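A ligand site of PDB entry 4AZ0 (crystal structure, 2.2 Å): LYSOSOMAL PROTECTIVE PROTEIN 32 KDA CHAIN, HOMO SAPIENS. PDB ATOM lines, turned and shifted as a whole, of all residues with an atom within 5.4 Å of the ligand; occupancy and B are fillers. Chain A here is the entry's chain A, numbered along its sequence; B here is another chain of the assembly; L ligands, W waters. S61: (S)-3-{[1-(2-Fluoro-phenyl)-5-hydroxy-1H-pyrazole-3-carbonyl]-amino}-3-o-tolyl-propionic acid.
The side-chain amide nitrogen of Asn 57 sits at hydrogen-bond distance from an oxygen (O27) of the ligand, 2.8 Å away.
The backbone NH of Gly 58 lies within hydrogen-bond range of an oxygen (O27) of the ligand (2.8 Å).
NE2 of His 131 of chain B sits at hydrogen-bond distance from O19 of the ligand (3.2 Å).
An oxygen (O19) of the ligand lies close to the side-chain carboxylate (OE2) of Glu 151, at 2.7 Å.
N9 of the ligand is in hydrogen-bond range of SG of Cys 62, 3.4 Å away.
OH of Tyr 249 is in hydrogen-bond range of O28 of the ligand, 3.3 Å away.
O of Ser 63 sits close to OD1 of Asn 57 (3.4 Å).
NE2 of His 131 of chain B sits at hydrogen-bond distance from OG of Ser 152 (2.9 Å).
N of His 131 of chain B sits at hydrogen-bond distance from O of Tyr 249, at 2.7 Å.
The backbone carbonyl oxygen of Pro 60 sits close to the side-chain amide oxygen of Asn 41 of chain B, 2.9 Å away.
O of Met 35 of chain B sits at hydrogen-bond distance from N of Ser 63, at 2.8 Å.
OE1 of Glu 151 lies close to OE1 of Glu 71, at 2.5 Å.
The side-chain amide nitrogen (ND2) of Asn 57 is in hydrogen-bond range of the side-chain carboxylate (OE2) of Glu 71, 3.1 Å away.
The backbone carbonyl oxygen (O) of Glu 151 sits at hydrogen-bond distance from the backbone NH (N) of Gly 58, 3.2 Å away.
N of Pro 3 of chain B sits close to F8 of the ligand (3.4 Å).
Gly 59 touches the ligand.
O of Pro 60 touches C4 of the ligand, 3.6 Å away.
OD1 of Asp 66 touches C23 of the ligand (3.5 Å).
Ser 152 touches the ligand (CB to O19, 3.6 Å).
Met 35 of chain B touches the ligand.
Cys 36 of chain B touches the ligand.
Asn 37 of chain B touches the ligand.
CA of Phe 38 of chain B touches C2 of the ligand, at 3.7 Å.
Asn 41 of chain B touches the ligand (CB to C3, 3.6 Å).
Hydrophobic or aromatic side chains within 4 Å of the ligand: Tyr 249, Pro 3 of chain B, Met 35 of chain B and His 131 of chain B.
Within 4 Å of the ligand: Asn 57, Gly 58, Gly 59, Pro 60, Cys 62, Asp 66, Glu 151, Ser 152, Tyr 249, Pro 3 of chain B, Met 35 of chain B, Cys 36 of chain B, Asn 37 of chain B, Phe 38 of chain B, Asn 41 of chain B and His 131 of chain B.
The nearest printed residue that does not touch the ligand is Thr 6 of chain B (4.1 Å).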
ATOM      1  N   LEU A  56      -2.839  21.673 -10.497  1.00  0.00           N
ATOM      2  CA  LEU A  56      -4.238  21.757 -10.070  1.00  0.00           C
ATOM      3  C   LEU A  56      -5.195  21.521 -11.223  1.00  0.00           C
ATOM      4  O   LEU A  56      -5.118  22.217 -12.235  1.00  0.00           O
ATOM      5  CB  LEU A  56      -4.537  23.111  -9.407  1.00  0.00           C
ATOM      6  CG  LEU A  56      -3.820  23.474  -8.105  1.00  0.00           C
ATOM      7  CD1 LEU A  56      -4.156  24.899  -7.687  1.00  0.00           C
ATOM      8  CD2 LEU A  56      -4.167  22.513  -6.976  1.00  0.00           C
ATOM      9  N   ASN A  57      -6.116  20.563 -11.066  1.00  0.00           N
ATOM     10  CA  ASN A  57      -7.168  20.367 -12.062  1.00  0.00           C
ATOM     11  C   ASN A  57      -8.321  21.306 -11.692  1.00  0.00           C
ATOM     12  O   ASN A  57      -8.354  21.821 -10.574  1.00  0.00           O
ATOM     13  CB  ASN A  57      -7.583  18.893 -12.161  1.00  0.00           C
ATOM     14  CG  ASN A  57      -6.748  18.120 -13.153  1.00  0.00           C
ATOM     15  OD1 ASN A  57      -5.856  17.357 -12.783  1.00  0.00           O
ATOM     16  ND2 ASN A  57      -6.971  18.325 -14.447  1.00  0.00           N
ATOM     17  N   GLY A  58      -9.215  21.572 -12.635  1.00  0.00           N
ATOM     18  CA  GLY A  58     -10.307  22.519 -12.442  1.00  0.00           C
ATOM     19  C   GLY A  58     -11.592  22.002 -11.851  1.00  0.00           C
ATOM     20  O   GLY A  58     -11.605  21.403 -10.772  1.00  0.00           O
ATOM     21  N   GLY A  59     -12.696  22.299 -12.555  1.00  0.00           N
ATOM     22  CA  GLY A  59     -14.044  21.947 -12.157  1.00  0.00           C
ATOM     23  C   GLY A  59     -14.919  23.185 -12.073  1.00  0.00           C
ATOM     24  O   GLY A  59     -15.469  23.598 -13.088  1.00  0.00           O
ATOM     25  N   PRO A  60     -15.055  23.841 -10.897  1.00  0.00           N
ATOM     26  CA  PRO A  60     -14.488  23.498  -9.569  1.00  0.00           C
ATOM     27  C   PRO A  60     -15.022  22.171  -9.062  1.00  0.00           C
ATOM     28  O   PRO A  60     -16.160  21.812  -9.364  1.00  0.00           O
ATOM     29  CB  PRO A  60     -14.964  24.648  -8.671  1.00  0.00           C
ATOM     30  CG  PRO A  60     -15.384  25.745  -9.583  1.00  0.00           C
ATOM     31  CD  PRO A  60     -15.890  25.051 -10.808  1.00  0.00           C
ATOM     32  N   GLY A  61     -14.194  21.434  -8.326  1.00  0.00           N
ATOM     33  CA  GLY A  61     -14.583  20.147  -7.756  1.00  0.00           C
ATOM     34  C   GLY A  61     -13.937  18.915  -8.368  1.00  0.00           C
ATOM     35  O   GLY A  61     -14.205  17.809  -7.896  1.00  0.00           O
ATOM     36  N   CYS A  62     -13.110  19.076  -9.406  1.00  0.00           N
ATOM     37  CA  CYS A  62     -12.443  17.934 -10.050  1.00  0.00           C
ATOM     38  C   CYS A  62     -11.052  17.670  -9.485  1.00  0.00           C
ATOM     39  O   CYS A  62     -10.352  18.600  -9.089  1.00  0.00           O
ATOM     40  CB  CYS A  62     -12.443  18.073 -11.564  1.00  0.00           C
ATOM     41  SG  CYS A  62     -14.094  18.154 -12.306  1.00  0.00           S
ATOM     42  N   SER A  63     -10.667  16.381  -9.420  1.00  0.00           N
ATOM     43  CA  SER A  63      -9.421  15.916  -8.841  1.00  0.00           C
ATOM     44  C   SER A  63      -8.162  16.077  -9.688  1.00  0.00           C
ATOM     45  O   SER A  63      -8.150  15.719 -10.862  1.00  0.00           O
ATOM     46  CB  SER A  63      -9.552  14.471  -8.380  1.00  0.00           C
ATOM     47  OG  SER A  63      -8.312  13.955  -7.916  1.00  0.00           O
ATOM     48  N   ASP A  66      -6.494  13.081 -11.747  1.00  0.00           N
ATOM     49  CA  ASP A  66      -6.844  12.902 -13.161  1.00  0.00           C
ATOM     50  C   ASP A  66      -5.609  13.296 -13.966  1.00  0.00           C
ATOM     51  O   ASP A  66      -5.230  12.582 -14.878  1.00  0.00           O
ATOM     52  CB  ASP A  66      -8.010  13.817 -13.565  1.00  0.00           C
ATOM     53  CG  ASP A  66      -8.236  13.918 -15.067  1.00  0.00           C
ATOM     54  OD1 ASP A  66      -8.831  12.979 -15.644  1.00  0.00           O
ATOM     55  OD2 ASP A  66      -7.800  14.929 -15.665  1.00  0.00           O
ATOM     56  N   GLU A  71      -3.228  12.310 -17.603  1.00  0.00           N
ATOM     57  CA  GLU A  71      -2.568  13.380 -18.366  1.00  0.00           C
ATOM     58  C   GLU A  71      -1.050  13.317 -18.479  1.00  0.00           C
ATOM     59  O   GLU A  71      -0.547  12.877 -19.521  1.00  0.00           O
ATOM     60  CB  GLU A  71      -3.018  14.769 -17.911  1.00  0.00           C
ATOM     61  CG  GLU A  71      -4.511  15.006 -17.933  1.00  0.00           C
ATOM     62  CD  GLU A  71      -4.866  16.455 -17.682  1.00  0.00           C
ATOM     63  OE1 GLU A  71      -4.679  17.267 -18.605  1.00  0.00           O
ATOM     64  OE2 GLU A  71      -5.280  16.779 -16.551  1.00  0.00           O
ATOM     65  N   GLU A 151      -5.067  23.513 -14.925  1.00  0.00           N
ATOM     66  CA  GLU A 151      -5.975  23.351 -16.058  1.00  0.00           C
ATOM     67  C   GLU A 151      -7.402  23.836 -15.767  1.00  0.00           C
ATOM     68  O   GLU A 151      -7.891  23.702 -14.652  1.00  0.00           O
ATOM     69  CB  GLU A 151      -6.006  21.864 -16.422  1.00  0.00           C
ATOM     70  CG  GLU A 151      -6.623  21.533 -17.760  1.00  0.00           C
ATOM     71  CD  GLU A 151      -6.409  20.073 -18.106  1.00  0.00           C
ATOM     72  OE1 GLU A 151      -5.264  19.720 -18.486  1.00  0.00           O
ATOM     73  OE2 GLU A 151      -7.359  19.277 -17.942  1.00  0.00           O
ATOM     74  N   SER A 152      -8.085  24.324 -16.824  1.00  0.00           N
ATOM     75  CA  SER A 152      -9.486  24.746 -16.831  1.00  0.00           C
ATOM     76  C   SER A 152      -9.813  25.819 -15.791  1.00  0.00           C
ATOM     77  O   SER A 152      -9.307  26.930 -15.922  1.00  0.00           O
ATOM     78  CB  SER A 152     -10.403  23.523 -16.741  1.00  0.00           C
ATOM     79  OG  SER A 152     -11.652  23.744 -17.374  1.00  0.00           O
ATOM     80  N   TYR A 249     -14.875  18.921 -25.006  1.00  0.00           N
ATOM     81  CA  TYR A 249     -13.465  18.887 -24.612  1.00  0.00           C
ATOM     82  C   TYR A 249     -12.493  18.603 -25.761  1.00  0.00           C
ATOM     83  O   TYR A 249     -11.319  18.938 -25.655  1.00  0.00           O
ATOM     84  CB  TYR A 249     -13.258  17.956 -23.406  1.00  0.00           C
ATOM     85  CG  TYR A 249     -14.135  18.332 -22.231  1.00  0.00           C
ATOM     86  CD1 TYR A 249     -13.916  19.506 -21.516  1.00  0.00           C
ATOM     87  CD2 TYR A 249     -15.224  17.534 -21.863  1.00  0.00           C
ATOM     88  CE1 TYR A 249     -14.736  19.867 -20.444  1.00  0.00           C
ATOM     89  CE2 TYR A 249     -16.037  17.877 -20.789  1.00  0.00           C
ATOM     90  CZ  TYR A 249     -15.798  19.057 -20.081  1.00  0.00           C
ATOM     91  OH  TYR A 249     -16.604  19.399 -19.027  1.00  0.00           O
ATOM     92  N   PRO B   3     -18.368  15.025 -15.838  1.00  0.00           N
ATOM     93  CA  PRO B   3     -18.558  15.893 -16.999  1.00  0.00           C
ATOM     94  C   PRO B   3     -18.993  15.125 -18.256  1.00  0.00           C
ATOM     95  O   PRO B   3     -18.559  13.982 -18.436  1.00  0.00           O
ATOM     96  CB  PRO B   3     -17.196  16.568 -17.187  1.00  0.00           C
ATOM     97  CG  PRO B   3     -16.226  15.688 -16.472  1.00  0.00           C
ATOM     98  CD  PRO B   3     -16.978  15.074 -15.333  1.00  0.00           C
ATOM     99  N   PRO B   4     -19.845  15.715 -19.131  1.00  0.00           N
ATOM    100  CA  PRO B   4     -20.318  14.995 -20.331  1.00  0.00           C
ATOM    101  C   PRO B   4     -19.233  14.610 -21.335  1.00  0.00           C
ATOM    102  O   PRO B   4     -18.190  15.279 -21.425  1.00  0.00           O
ATOM    103  CB  PRO B   4     -21.348  15.941 -20.949  1.00  0.00           C
ATOM    104  CG  PRO B   4     -21.735  16.873 -19.843  1.00  0.00           C
ATOM    105  CD  PRO B   4     -20.478  17.052 -19.045  1.00  0.00           C
ATOM    106  N   THR B   6     -17.062  12.313 -21.329  1.00  0.00           N
ATOM    107  CA  THR B   6     -15.826  11.813 -20.739  1.00  0.00           C
ATOM    108  C   THR B   6     -16.059  10.496 -20.011  1.00  0.00           C
ATOM    109  O   THR B   6     -17.096  10.337 -19.344  1.00  0.00           O
ATOM    110  CB  THR B   6     -15.189  12.840 -19.780  1.00  0.00           C
ATOM    111  OG1 THR B   6     -16.062  13.059 -18.663  1.00  0.00           O
ATOM    112  CG2 THR B   6     -14.851  14.158 -20.462  1.00  0.00           C
ATOM    113  N   THR B   8     -14.411   8.318 -17.154  1.00  0.00           N
ATOM    114  CA  THR B   8     -13.475   8.361 -16.021  1.00  0.00           C
ATOM    115  C   THR B   8     -13.386   7.028 -15.253  1.00  0.00           C
ATOM    116  O   THR B   8     -12.669   6.964 -14.241  1.00  0.00           O
ATOM    117  CB  THR B   8     -13.803   9.556 -15.110  1.00  0.00           C
ATOM    118  OG1 THR B   8     -15.053   9.320 -14.439  1.00  0.00           O
ATOM    119  CG2 THR B   8     -13.846  10.887 -15.862  1.00  0.00           C
ATOM    120  N   MET B  35     -14.096  11.386  -9.594  1.00  0.00           N
ATOM    121  CA  MET B  35     -13.268  12.258 -10.449  1.00  0.00           C
ATOM    122  C   MET B  35     -13.603  13.734 -10.215  1.00  0.00           C
ATOM    123  O   MET B  35     -12.706  14.547 -10.034  1.00  0.00           O
ATOM    124  CB  MET B  35     -13.453  11.872 -11.931  1.00  0.00           C
ATOM    125  CG  MET B  35     -12.608  12.694 -12.894  1.00  0.00           C
ATOM    126  SD  MET B  35     -10.833  12.431 -12.717  1.00  0.00           S
ATOM    127  CE  MET B  35     -10.615  10.933 -13.672  1.00  0.00           C
ATOM    128  N   CYS B  36     -14.904  14.048 -10.177  1.00  0.00           N
ATOM    129  CA  CYS B  36     -15.428  15.380  -9.945  1.00  0.00           C
ATOM    130  C   CYS B  36     -16.504  15.328  -8.857  1.00  0.00           C
ATOM    131  O   CYS B  36     -17.417  14.501  -8.944  1.00  0.00           O
ATOM    132  CB  CYS B  36     -15.965  15.974 -11.246  1.00  0.00           C
ATOM    133  SG  CYS B  36     -14.699  16.219 -12.531  1.00  0.00           S
ATOM    134  N   ASN B  37     -16.374  16.179  -7.833  1.00  0.00           N
ATOM    135  CA  ASN B  37     -17.332  16.238  -6.720  1.00  0.00           C
ATOM    136  C   ASN B  37     -18.444  17.238  -7.041  1.00  0.00           C
ATOM    137  O   ASN B  37     -18.222  18.453  -6.986  1.00  0.00           O
ATOM    138  CB  ASN B  37     -16.629  16.577  -5.395  1.00  0.00           C
ATOM    139  CG  ASN B  37     -17.470  16.319  -4.168  1.00  0.00           C
ATOM    140  OD1 ASN B  37     -18.577  16.849  -4.009  1.00  0.00           O
ATOM    141  ND2 ASN B  37     -16.931  15.557  -3.238  1.00  0.00           N
ATOM    142  N   PHE B  38     -19.630  16.715  -7.395  1.00  0.00           N
ATOM    143  CA  PHE B  38     -20.818  17.489  -7.753  1.00  0.00           C
ATOM    144  C   PHE B  38     -21.262  18.453  -6.653  1.00  0.00           C
ATOM    145  O   PHE B  38     -21.635  19.594  -6.963  1.00  0.00           O
ATOM    146  CB  PHE B  38     -21.961  16.553  -8.183  1.00  0.00           C
ATOM    147  CG  PHE B  38     -23.331  17.172  -8.328  1.00  0.00           C
ATOM    148  CD1 PHE B  38     -23.577  18.142  -9.297  1.00  0.00           C
ATOM    149  CD2 PHE B  38     -24.386  16.757  -7.522  1.00  0.00           C
ATOM    150  CE1 PHE B  38     -24.853  18.710  -9.433  1.00  0.00           C
ATOM    151  CE2 PHE B  38     -25.655  17.327  -7.665  1.00  0.00           C
ATOM    152  CZ  PHE B  38     -25.878  18.296  -8.626  1.00  0.00           C
ATOM    153  N   ASN B  41     -18.928  21.549  -6.466  1.00  0.00           N
ATOM    154  CA  ASN B  41     -19.239  22.419  -7.603  1.00  0.00           C
ATOM    155  C   ASN B  41     -20.515  23.231  -7.363  1.00  0.00           C
ATOM    156  O   ASN B  41     -20.517  24.432  -7.599  1.00  0.00           O
ATOM    157  CB  ASN B  41     -19.369  21.597  -8.887  1.00  0.00           C
ATOM    158  CG  ASN B  41     -19.503  22.430 -10.143  1.00  0.00           C
ATOM    159  OD1 ASN B  41     -18.525  22.795 -10.795  1.00  0.00           O
ATOM    160  ND2 ASN B  41     -20.740  22.733 -10.522  1.00  0.00           N
ATOM    161  N   ALA B  76     -14.626  23.992 -24.434  1.00  0.00           N
ATOM    162  CA  ALA B  76     -14.912  24.428 -23.056  1.00  0.00           C
ATOM    163  C   ALA B  76     -14.177  25.738 -22.728  1.00  0.00           C
ATOM    164  O   ALA B  76     -14.811  26.716 -22.355  1.00  0.00           O
ATOM    165  CB  ALA B  76     -14.534  23.327 -22.060  1.00  0.00           C
ATOM    166  N   HIS B 131      -9.053  19.771 -24.560  1.00  0.00           N
ATOM    167  CA  HIS B 131      -9.033  20.276 -23.183  1.00  0.00           C
ATOM    168  C   HIS B 131      -7.876  19.737 -22.355  1.00  0.00           C
ATOM    169  O   HIS B 131      -7.292  20.486 -21.562  1.00  0.00           O
ATOM    170  CB  HIS B 131     -10.362  19.969 -22.505  1.00  0.00           C
ATOM    171  CG  HIS B 131     -10.680  20.838 -21.332  1.00  0.00           C
ATOM    172  ND1 HIS B 131     -10.854  22.204 -21.472  1.00  0.00           N
ATOM    173  CD2 HIS B 131     -10.895  20.495 -20.041  1.00  0.00           C
ATOM    174  CE1 HIS B 131     -11.145  22.648 -20.267  1.00  0.00           C
ATOM    175  NE2 HIS B 131     -11.192  21.657 -19.375  1.00  0.00           N
ATOM    176  N   MET B 132      -7.565  18.435 -22.505  1.00  0.00           N
ATOM    177  CA  MET B 132      -6.468  17.784 -21.786  1.00  0.00           C
ATOM    178  C   MET B 132      -5.303  17.597 -22.742  1.00  0.00           C
ATOM    179  O   MET B 132      -5.113  16.527 -23.308  1.00  0.00           O
ATOM    180  CB  MET B 132      -6.936  16.467 -21.143  1.00  0.00           C
ATOM    181  CG  MET B 132      -7.890  16.684 -19.979  1.00  0.00           C
ATOM    182  SD  MET B 132      -8.404  15.172 -19.142  1.00  0.00           S
ATOM    183  CE  MET B 132      -9.569  14.532 -20.343  1.00  0.00           C
HETATM  184  C26 S61 L   1     -13.304  17.239 -18.186  1.00  0.00           C
HETATM  185  C25 S61 L   1     -12.617  16.770 -16.924  1.00  0.00           C
HETATM  186  C24 S61 L   1     -12.411  15.400 -16.740  1.00  0.00           C
HETATM  187  C23 S61 L   1     -11.736  14.916 -15.634  1.00  0.00           C
HETATM  188  C22 S61 L   1     -11.261  15.786 -14.681  1.00  0.00           C
HETATM  189  C21 S61 L   1     -11.451  17.155 -14.836  1.00  0.00           C
HETATM  190  C20 S61 L   1     -12.132  17.658 -15.944  1.00  0.00           C
HETATM  191  C16 S61 L   1     -12.314  19.169 -16.103  1.00  0.00           C
HETATM  192  C17 S61 L   1     -11.367  20.122 -15.339  1.00  0.00           C
HETATM  193  C18 S61 L   1      -9.930  20.080 -15.791  1.00  0.00           C
HETATM  194  O27 S61 L   1      -8.998  20.117 -15.014  1.00  0.00           O
HETATM  195  O19 S61 L   1      -9.771  20.017 -17.084  1.00  0.00           O
HETATM  196  N15 S61 L   1     -13.700  19.463 -15.744  1.00  0.00           N
HETATM  197  C14 S61 L   1     -14.535  20.350 -16.299  1.00  0.00           C
HETATM  198  O28 S61 L   1     -14.254  21.003 -17.307  1.00  0.00           O
HETATM  199  C10 S61 L   1     -15.839  20.538 -15.604  1.00  0.00           C
HETATM  200  N9  S61 L   1     -16.084  19.636 -14.629  1.00  0.00           N
HETATM  201  C11 S61 L   1     -16.886  21.471 -15.722  1.00  0.00           C
HETATM  202  C12 S61 L   1     -17.835  21.123 -14.786  1.00  0.00           C
HETATM  203  O13 S61 L   1     -19.038  21.614 -14.419  1.00  0.00           O
HETATM  204  N7  S61 L   1     -17.315  20.006 -14.133  1.00  0.00           N
HETATM  205  C5  S61 L   1     -17.880  19.246 -13.071  1.00  0.00           C
HETATM  206  C4  S61 L   1     -17.502  19.509 -11.753  1.00  0.00           C
HETATM  207  C3  S61 L   1     -18.100  18.820 -10.707  1.00  0.00           C
HETATM  208  C2  S61 L   1     -19.071  17.855 -10.950  1.00  0.00           C
HETATM  209  C1  S61 L   1     -19.456  17.571 -12.251  1.00  0.00           C
HETATM  210  C6  S61 L   1     -18.864  18.259 -13.275  1.00  0.00           C
HETATM  211  F8  S61 L   1     -19.247  17.991 -14.543  1.00  0.00           F
HETATM  212  O   HOH W   1     -15.267  23.182 -18.613  1.00  0.00           O
HETATM  213  O   HOH W   2     -11.285  12.281 -17.844  1.00  0.00           O
